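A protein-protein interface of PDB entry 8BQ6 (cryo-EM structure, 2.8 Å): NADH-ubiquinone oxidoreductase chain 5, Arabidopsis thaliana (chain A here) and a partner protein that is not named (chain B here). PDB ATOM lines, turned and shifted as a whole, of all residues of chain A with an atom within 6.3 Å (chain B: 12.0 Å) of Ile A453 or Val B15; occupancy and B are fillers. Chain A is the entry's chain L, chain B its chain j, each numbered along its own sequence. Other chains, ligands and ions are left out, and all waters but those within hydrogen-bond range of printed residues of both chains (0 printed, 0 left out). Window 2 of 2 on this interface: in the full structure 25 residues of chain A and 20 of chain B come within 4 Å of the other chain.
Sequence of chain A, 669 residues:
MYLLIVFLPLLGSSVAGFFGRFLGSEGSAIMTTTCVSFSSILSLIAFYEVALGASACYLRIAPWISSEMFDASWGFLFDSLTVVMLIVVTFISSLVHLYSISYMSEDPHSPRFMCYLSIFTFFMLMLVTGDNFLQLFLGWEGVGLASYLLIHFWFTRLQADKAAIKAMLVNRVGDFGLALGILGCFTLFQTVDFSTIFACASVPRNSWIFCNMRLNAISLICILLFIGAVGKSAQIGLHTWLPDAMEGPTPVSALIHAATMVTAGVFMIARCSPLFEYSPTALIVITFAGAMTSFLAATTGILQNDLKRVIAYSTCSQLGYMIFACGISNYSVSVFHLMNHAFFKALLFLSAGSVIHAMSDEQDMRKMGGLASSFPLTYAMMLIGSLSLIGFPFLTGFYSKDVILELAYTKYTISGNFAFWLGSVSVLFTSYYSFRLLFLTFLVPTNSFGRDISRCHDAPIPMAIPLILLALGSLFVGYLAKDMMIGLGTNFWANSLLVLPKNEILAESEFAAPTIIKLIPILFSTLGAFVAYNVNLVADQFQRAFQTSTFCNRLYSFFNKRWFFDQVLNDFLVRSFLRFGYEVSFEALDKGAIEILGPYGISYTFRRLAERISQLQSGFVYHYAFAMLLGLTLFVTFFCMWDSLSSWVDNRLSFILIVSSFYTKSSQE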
ATOM      1  N   MET A 359     -18.115 -19.643  30.642  1.00  0.00           N
ATOM      2  CA  MET A 359     -18.956 -18.745  29.864  1.00  0.00           C
ATOM      3  C   MET A 359     -18.493 -17.297  29.944  1.00  0.00           C
ATOM      4  O   MET A 359     -19.317 -16.380  29.858  1.00  0.00           O
ATOM      5  CB  MET A 359     -20.408 -18.867  30.319  1.00  0.00           C
ATOM      6  CG  MET A 359     -21.028 -20.201  29.969  1.00  0.00           C
ATOM      7  SD  MET A 359     -21.327 -20.361  28.201  1.00  0.00           S
ATOM      8  CE  MET A 359     -22.585 -19.111  27.975  1.00  0.00           C
ATOM      9  N   GLY A 369     -28.085 -21.983  28.688  1.00  0.00           N
ATOM     10  CA  GLY A 369     -28.952 -23.022  28.177  1.00  0.00           C
ATOM     11  C   GLY A 369     -28.314 -23.753  27.011  1.00  0.00           C
ATOM     12  O   GLY A 369     -27.616 -23.165  26.177  1.00  0.00           O
ATOM     13  N   GLY A 370     -28.580 -25.053  26.934  1.00  0.00           N
ATOM     14  CA  GLY A 370     -27.889 -25.880  25.959  1.00  0.00           C
ATOM     15  C   GLY A 370     -26.422 -26.076  26.268  1.00  0.00           C
ATOM     16  O   GLY A 370     -25.589 -26.086  25.352  1.00  0.00           O
ATOM     17  N   LEU A 371     -26.087 -26.247  27.548  1.00  0.00           N
ATOM     18  CA  LEU A 371     -24.712 -26.418  27.999  1.00  0.00           C
ATOM     19  C   LEU A 371     -24.424 -27.799  28.573  1.00  0.00           C
ATOM     20  O   LEU A 371     -23.298 -28.041  29.017  1.00  0.00           O
ATOM     21  CB  LEU A 371     -24.364 -25.357  29.051  1.00  0.00           C
ATOM     22  CG  LEU A 371     -23.901 -23.949  28.670  1.00  0.00           C
ATOM     23  CD1 LEU A 371     -24.605 -23.388  27.446  1.00  0.00           C
ATOM     24  CD2 LEU A 371     -24.128 -23.047  29.862  1.00  0.00           C
ATOM     25  N   SER A 374     -21.990 -29.389  26.139  1.00  0.00           N
ATOM     26  CA  SER A 374     -20.745 -28.637  26.044  1.00  0.00           C
ATOM     27  C   SER A 374     -19.877 -28.818  27.283  1.00  0.00           C
ATOM     28  O   SER A 374     -18.647 -28.860  27.168  1.00  0.00           O
ATOM     29  CB  SER A 374     -21.039 -27.157  25.802  1.00  0.00           C
ATOM     30  OG  SER A 374     -21.142 -26.448  27.019  1.00  0.00           O
ATOM     31  N   PHE A 375     -20.490 -28.947  28.465  1.00  0.00           N
ATOM     32  CA  PHE A 375     -19.780 -29.152  29.727  1.00  0.00           C
ATOM     33  C   PHE A 375     -20.349 -30.397  30.395  1.00  0.00           C
ATOM     34  O   PHE A 375     -21.189 -30.302  31.304  1.00  0.00           O
ATOM     35  CB  PHE A 375     -19.899 -27.935  30.641  1.00  0.00           C
ATOM     36  CG  PHE A 375     -19.719 -26.636  29.928  1.00  0.00           C
ATOM     37  CD1 PHE A 375     -18.585 -26.402  29.175  1.00  0.00           C
ATOM     38  CD2 PHE A 375     -20.688 -25.655  29.994  1.00  0.00           C
ATOM     39  CE1 PHE A 375     -18.418 -25.215  28.508  1.00  0.00           C
ATOM     40  CE2 PHE A 375     -20.524 -24.463  29.331  1.00  0.00           C
ATOM     41  CZ  PHE A 375     -19.389 -24.242  28.586  1.00  0.00           C
ATOM     42  N   THR A 446     -30.518 -23.034  23.738  1.00  0.00           N
ATOM     43  CA  THR A 446     -29.571 -22.002  24.142  1.00  0.00           C
ATOM     44  C   THR A 446     -30.180 -20.614  24.049  1.00  0.00           C
ATOM     45  O   THR A 446     -30.804 -20.250  23.048  1.00  0.00           O
ATOM     46  CB  THR A 446     -28.309 -22.046  23.279  1.00  0.00           C
ATOM     47  OG1 THR A 446     -28.495 -21.216  22.127  1.00  0.00           O
ATOM     48  CG2 THR A 446     -28.009 -23.458  22.839  1.00  0.00           C
ATOM     49  N   SER A 448     -28.106 -17.923  24.753  1.00  0.00           N
ATOM     50  CA  SER A 448     -26.845 -17.285  25.072  1.00  0.00           C
ATOM     51  C   SER A 448     -26.249 -16.594  23.845  1.00  0.00           C
ATOM     52  O   SER A 448     -26.791 -16.649  22.739  1.00  0.00           O
ATOM     53  CB  SER A 448     -25.895 -18.325  25.663  1.00  0.00           C
ATOM     54  OG  SER A 448     -25.229 -19.053  24.650  1.00  0.00           O
ATOM     55  N   PHE A 449     -25.120 -15.920  24.055  1.00  0.00           N
ATOM     56  CA  PHE A 449     -24.413 -15.213  22.995  1.00  0.00           C
ATOM     57  C   PHE A 449     -23.416 -16.138  22.311  1.00  0.00           C
ATOM     58  O   PHE A 449     -22.811 -17.002  22.950  1.00  0.00           O
ATOM     59  CB  PHE A 449     -23.682 -13.990  23.551  1.00  0.00           C
ATOM     60  CG  PHE A 449     -24.592 -12.935  24.101  1.00  0.00           C
ATOM     61  CD1 PHE A 449     -25.160 -11.987  23.270  1.00  0.00           C
ATOM     62  CD2 PHE A 449     -24.875 -12.885  25.453  1.00  0.00           C
ATOM     63  CE1 PHE A 449     -25.993 -11.014  23.777  1.00  0.00           C
ATOM     64  CE2 PHE A 449     -25.710 -11.915  25.962  1.00  0.00           C
ATOM     65  CZ  PHE A 449     -26.271 -10.980  25.123  1.00  0.00           C
ATOM     66  N   GLY A 450     -23.238 -15.936  21.004  1.00  0.00           N
ATOM     67  CA  GLY A 450     -22.367 -16.814  20.238  1.00  0.00           C
ATOM     68  C   GLY A 450     -20.910 -16.722  20.646  1.00  0.00           C
ATOM     69  O   GLY A 450     -20.212 -17.737  20.721  1.00  0.00           O
ATOM     70  N   ARG A 451     -20.428 -15.505  20.912  1.00  0.00           N
ATOM     71  CA  ARG A 451     -19.021 -15.328  21.253  1.00  0.00           C
ATOM     72  C   ARG A 451     -18.656 -16.051  22.544  1.00  0.00           C
ATOM     73  O   ARG A 451     -17.500 -16.449  22.725  1.00  0.00           O
ATOM     74  CB  ARG A 451     -18.694 -13.839  21.353  1.00  0.00           C
ATOM     75  CG  ARG A 451     -19.196 -13.164  22.613  1.00  0.00           C
ATOM     76  CD  ARG A 451     -18.672 -11.743  22.713  1.00  0.00           C
ATOM     77  NE  ARG A 451     -17.231 -11.661  22.515  1.00  0.00           N
ATOM     78  CZ  ARG A 451     -16.333 -11.882  23.466  1.00  0.00           C
ATOM     79  NH1 ARG A 451     -16.696 -12.210  24.695  1.00  0.00           N
ATOM     80  NH2 ARG A 451     -15.041 -11.768  23.176  1.00  0.00           N
ATOM     81  N   ASP A 452     -19.621 -16.229  23.449  1.00  0.00           N
ATOM     82  CA  ASP A 452     -19.360 -17.007  24.655  1.00  0.00           C
ATOM     83  C   ASP A 452     -19.291 -18.495  24.339  1.00  0.00           C
ATOM     84  O   ASP A 452     -18.422 -19.208  24.853  1.00  0.00           O
ATOM     85  CB  ASP A 452     -20.445 -16.736  25.698  1.00  0.00           C
ATOM     86  CG  ASP A 452     -20.402 -15.318  26.245  1.00  0.00           C
ATOM     87  OD1 ASP A 452     -19.304 -14.725  26.321  1.00  0.00           O
ATOM     88  OD2 ASP A 452     -21.478 -14.795  26.603  1.00  0.00           O
ATOM     89  N   ILE A 453     -20.198 -18.975  23.483  1.00  0.00           N
ATOM     90  CA  ILE A 453     -20.270 -20.398  23.161  1.00  0.00           C
ATOM     91  C   ILE A 453     -19.014 -20.848  22.431  1.00  0.00           C
ATOM     92  O   ILE A 453     -18.504 -21.952  22.655  1.00  0.00           O
ATOM     93  CB  ILE A 453     -21.543 -20.685  22.343  1.00  0.00           C
ATOM     94  CG1 ILE A 453     -22.759 -20.752  23.265  1.00  0.00           C
ATOM     95  CG2 ILE A 453     -21.412 -21.976  21.561  1.00  0.00           C
ATOM     96  CD1 ILE A 453     -22.555 -21.645  24.459  1.00  0.00           C
ATOM     97  N   SER A 454     -18.487 -19.997  21.557  1.00  0.00           N
ATOM     98  CA  SER A 454     -17.288 -20.313  20.798  1.00  0.00           C
ATOM     99  C   SER A 454     -16.000 -20.068  21.576  1.00  0.00           C
ATOM    100  O   SER A 454     -14.918 -20.159  20.987  1.00  0.00           O
ATOM    101  CB  SER A 454     -17.280 -19.514  19.494  1.00  0.00           C
ATOM    102  OG  SER A 454     -17.839 -18.227  19.686  1.00  0.00           O
ATOM    103  N   ARG A 455     -16.080 -19.766  22.877  1.00  0.00           N
ATOM    104  CA  ARG A 455     -14.891 -19.648  23.716  1.00  0.00           C
ATOM    105  C   ARG A 455     -14.982 -20.534  24.956  1.00  0.00           C
ATOM    106  O   ARG A 455     -14.263 -20.301  25.932  1.00  0.00           O
ATOM    107  CB  ARG A 455     -14.648 -18.191  24.126  1.00  0.00           C
ATOM    108  CG  ARG A 455     -13.179 -17.770  24.093  1.00  0.00           C
ATOM    109  CD  ARG A 455     -13.001 -16.268  24.266  1.00  0.00           C
ATOM    110  NE  ARG A 455     -13.199 -15.841  25.647  1.00  0.00           N
ATOM    111  CZ  ARG A 455     -13.689 -14.663  26.003  1.00  0.00           C
ATOM    112  NH1 ARG A 455     -14.083 -13.777  25.104  1.00  0.00           N
ATOM    113  NH2 ARG A 455     -13.782 -14.362  27.296  1.00  0.00           N
ATOM    114  N   CYS A 456     -15.841 -21.547  24.935  1.00  0.00           N
ATOM    115  CA  CYS A 456     -16.065 -22.388  26.101  1.00  0.00           C
ATOM    116  C   CYS A 456     -14.919 -23.374  26.318  1.00  0.00           C
ATOM    117  O   CYS A 456     -14.230 -23.797  25.385  1.00  0.00           O
ATOM    118  CB  CYS A 456     -17.375 -23.160  25.964  1.00  0.00           C
ATOM    119  SG  CYS A 456     -18.865 -22.149  25.946  1.00  0.00           S
ATOM    120  N   GLY B   9     -13.276 -28.735  17.012  1.00  0.00           N
ATOM    121  CA  GLY B   9     -14.719 -28.818  17.138  1.00  0.00           C
ATOM    122  C   GLY B   9     -15.434 -28.772  15.803  1.00  0.00           C
ATOM    123  O   GLY B   9     -14.832 -29.027  14.760  1.00  0.00           O
ATOM    124  N   ILE B  10     -16.722 -28.441  15.840  1.00  0.00           N
ATOM    125  CA  ILE B  10     -17.565 -28.345  14.653  1.00  0.00           C
ATOM    126  C   ILE B  10     -18.047 -26.911  14.511  1.00  0.00           C
ATOM    127  O   ILE B  10     -18.453 -26.284  15.497  1.00  0.00           O
ATOM    128  CB  ILE B  10     -18.754 -29.320  14.726  1.00  0.00           C
ATOM    129  CG1 ILE B  10     -18.248 -30.751  14.903  1.00  0.00           C
ATOM    130  CG2 ILE B  10     -19.663 -29.176  13.503  1.00  0.00           C
ATOM    131  CD1 ILE B  10     -18.692 -31.393  16.179  1.00  0.00           C
ATOM    132  N   THR B  11     -17.993 -26.387  13.292  1.00  0.00           N
ATOM    133  CA  THR B  11     -18.491 -25.051  13.002  1.00  0.00           C
ATOM    134  C   THR B  11     -19.815 -25.162  12.270  1.00  0.00           C
ATOM    135  O   THR B  11     -19.915 -25.836  11.240  1.00  0.00           O
ATOM    136  CB  THR B  11     -17.498 -24.234  12.180  1.00  0.00           C
ATOM    137  OG1 THR B  11     -16.559 -23.609  13.061  1.00  0.00           O
ATOM    138  CG2 THR B  11     -18.225 -23.151  11.388  1.00  0.00           C
ATOM    139  N   TYR B  12     -20.822 -24.493  12.810  1.00  0.00           N
ATOM    140  CA  TYR B  12     -22.113 -24.337  12.162  1.00  0.00           C
ATOM    141  C   TYR B  12     -22.357 -22.837  12.081  1.00  0.00           C
ATOM    142  O   TYR B  12     -22.775 -22.218  13.065  1.00  0.00           O
ATOM    143  CB  TYR B  12     -23.192 -25.083  12.948  1.00  0.00           C
ATOM    144  CG  TYR B  12     -24.449 -25.454  12.199  1.00  0.00           C
ATOM    145  CD1 TYR B  12     -25.688 -25.056  12.664  1.00  0.00           C
ATOM    146  CD2 TYR B  12     -24.397 -26.200  11.028  1.00  0.00           C
ATOM    147  CE1 TYR B  12     -26.839 -25.411  12.011  1.00  0.00           C
ATOM    148  CE2 TYR B  12     -25.552 -26.539  10.348  1.00  0.00           C
ATOM    149  CZ  TYR B  12     -26.770 -26.136  10.843  1.00  0.00           C
ATOM    150  OH  TYR B  12     -27.931 -26.467  10.183  1.00  0.00           O
ATOM    151  N   LYS B  13     -22.002 -22.258  10.934  1.00  0.00           N
ATOM    152  CA  LYS B  13     -22.323 -20.881  10.519  1.00  0.00           C
ATOM    153  C   LYS B  13     -21.903 -19.829  11.544  1.00  0.00           C
ATOM    154  O   LYS B  13     -22.720 -19.232  12.245  1.00  0.00           O
ATOM    155  CB  LYS B  13     -23.797 -20.727  10.133  1.00  0.00           C
ATOM    156  CG  LYS B  13     -24.851 -21.133  11.126  1.00  0.00           C
ATOM    157  CD  LYS B  13     -26.123 -21.072  10.482  1.00  0.00           C
ATOM    158  CE  LYS B  13     -26.630 -22.397   9.973  1.00  0.00           C
ATOM    159  NZ  LYS B  13     -27.637 -22.903  10.936  1.00  0.00           N
ATOM    160  N   GLY B  14     -20.590 -19.628  11.636  1.00  0.00           N
ATOM    161  CA  GLY B  14     -20.043 -18.565  12.455  1.00  0.00           C
ATOM    162  C   GLY B  14     -19.726 -19.055  13.846  1.00  0.00           C
ATOM    163  O   GLY B  14     -18.594 -18.938  14.323  1.00  0.00           O
ATOM    164  N   VAL B  15     -20.724 -19.635  14.495  1.00  0.00           N
ATOM    165  CA  VAL B  15     -20.574 -20.106  15.865  1.00  0.00           C
ATOM    166  C   VAL B  15     -19.967 -21.502  15.841  1.00  0.00           C
ATOM    167  O   VAL B  15     -20.516 -22.423  15.227  1.00  0.00           O
ATOM    168  CB  VAL B  15     -21.928 -20.091  16.588  1.00  0.00           C
ATOM    169  CG1 VAL B  15     -21.785 -20.633  17.998  1.00  0.00           C
ATOM    170  CG2 VAL B  15     -22.502 -18.677  16.592  1.00  0.00           C
ATOM    171  N   THR B  16     -18.828 -21.657  16.507  1.00  0.00           N
ATOM    172  CA  THR B  16     -18.104 -22.918  16.567  1.00  0.00           C
ATOM    173  C   THR B  16     -18.235 -23.498  17.969  1.00  0.00           C
ATOM    174  O   THR B  16     -18.191 -22.759  18.959  1.00  0.00           O
ATOM    175  CB  THR B  16     -16.631 -22.716  16.174  1.00  0.00           C
ATOM    176  OG1 THR B  16     -16.067 -23.959  15.739  1.00  0.00           O
ATOM    177  CG2 THR B  16     -15.796 -22.144  17.322  1.00  0.00           C
ATOM    178  N   VAL B  17     -18.447 -24.806  18.055  1.00  0.00           N
ATOM    179  CA  VAL B  17     -18.507 -25.504  19.335  1.00  0.00           C
ATOM    180  C   VAL B  17     -17.359 -26.496  19.384  1.00  0.00           C
ATOM    181  O   VAL B  17     -17.196 -27.314  18.472  1.00  0.00           O
ATOM    182  CB  VAL B  17     -19.848 -26.224  19.547  1.00  0.00           C
ATOM    183  CG1 VAL B  17     -19.662 -27.374  20.528  1.00  0.00           C
ATOM    184  CG2 VAL B  17     -20.892 -25.261  20.061  1.00  0.00           C
ATOM    185  N   HIS B  18     -16.567 -26.423  20.446  1.00  0.00           N
ATOM    186  CA  HIS B  18     -15.478 -27.360  20.654  1.00  0.00           C
ATOM    187  C   HIS B  18     -15.985 -28.586  21.395  1.00  0.00           C
ATOM    188  O   HIS B  18     -16.751 -28.475  22.357  1.00  0.00           O
ATOM    189  CB  HIS B  18     -14.347 -26.700  21.437  1.00  0.00           C
ATOM    190  CG  HIS B  18     -14.088 -25.284  21.033  1.00  0.00           C
ATOM    191  ND1 HIS B  18     -14.659 -24.210  21.682  1.00  0.00           N
ATOM    192  CD2 HIS B  18     -13.329 -24.764  20.041  1.00  0.00           C
ATOM    193  CE1 HIS B  18     -14.257 -23.090  21.109  1.00  0.00           C
ATOM    194  NE2 HIS B  18     -13.448 -23.398  20.112  1.00  0.00           N
ATOM    195  N   THR B  19     -15.568 -29.754  20.929  1.00  0.00           N
ATOM    196  CA  THR B  19     -15.921 -30.982  21.612  1.00  0.00           C
ATOM    197  C   THR B  19     -15.264 -31.016  22.993  1.00  0.00           C
ATOM    198  O   THR B  19     -14.149 -30.513  23.167  1.00  0.00           O
ATOM    199  CB  THR B  19     -15.504 -32.196  20.771  1.00  0.00           C
ATOM    200  OG1 THR B  19     -16.220 -33.361  21.198  1.00  0.00           O
ATOM    201  CG2 THR B  19     -14.002 -32.445  20.850  1.00  0.00           C
ATOM    202  N   PRO B  20     -15.943 -31.552  24.001  1.00  0.00           N
ATOM    203  CA  PRO B  20     -15.333 -31.647  25.329  1.00  0.00           C
ATOM    204  C   PRO B  20     -14.201 -32.665  25.347  1.00  0.00           C
ATOM    205  O   PRO B  20     -14.112 -33.553  24.498  1.00  0.00           O
ATOM    206  CB  PRO B  20     -16.496 -32.089  26.222  1.00  0.00           C
ATOM    207  CG  PRO B  20     -17.425 -32.789  25.303  1.00  0.00           C
ATOM    208  CD  PRO B  20     -17.299 -32.124  23.968  1.00  0.00           C
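Ser A374 touches Pro B20. Val B15 touches Ile A453 (CG1 to CG2, 3.8 Å). Thr B16 touches Ile A453 (O to O, 3.8 Å). CG2 of Ile A453 touches CG2 of Val B17, 3.6 Å away. Ser A454 touches Thr B16. CE1 of His B18 touches O of Ser A454 (3.0 Å). Cys A456 touches His B18 (O to ND1, 3.8 Å).
The backbone carbonyl oxygen (O) of Leu A371 is in hydrogen-bond range of the side-chain hydroxyl (OG) of Ser A374. The side-chain sulfur of Met A359 sits at hydrogen-bond distance from the side-chain sulfur of Cys A456. The side-chain hydroxyl of Ser A454 sits at hydrogen-bond distance from the backbone carbonyl oxygen of Gly A450 (2.6 Å). The side-chain sulfur of Cys A456 lies within hydrogen-bond range of the backbone carbonyl oxygen of Asp A452 (3.2 Å). OG1 of Thr B16 is in hydrogen-bond range of O of Ile B10 (3.3 Å). The side-chain hydroxyl (OG1) of Thr B16 sits at hydrogen-bond distance from the side-chain hydroxyl (OG1) of Thr B11, at 2.7 Å.
Hydrophobic or aromatic side chains of chain A within 4 Å of the printed part of chain B: Ile A453. Of the 12 printed residues of chain B, 5 touch a printed residue of chain A. Hydrophobic or aromatic side chains of chain B that line the printed part of chain A: Val B15, Val B17, His B18 and Pro B20.
Ile A453 touches just these residues of chain B: Val B15, Thr B16 and Val B17. Printed residues of chain A within 4 Å of Val B15: Ile A453. No residue of chain B comes within 4 Å of Met A359. No residue of chain B comes within 4 Å of Gly A369. No residue of chain B comes within 4 Å of Gly A370. No residue of chain B comes within 4 Å of Leu A371. No residue of chain B comes within 4 Å of Ser A448. No residue of chain B comes within 4 Å of Gly A450. No residue of chain B comes within 4 Å of Asp A452. Cys A456 touches just one residue of chain B: His B18 (3.8 Å). Printed residues of chain A within 4 Å of Val B17: Ile A453. Of the printed residues of chain A, Thr B16 touches Ile A453 and Ser A454. Of the printed residues of chain A, His B18 touches Ser A454 and Cys A456. Of the printed residues of chain B, Ser A374 touches Pro B20 (3.99 Å). Tyr B12 touches none of the printed residues of chain A. Gly B14 touches none of the printed residues of chain A. The nearest residue of chain A that does not touch Val B15 is Gly A450 (4.1 Å).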
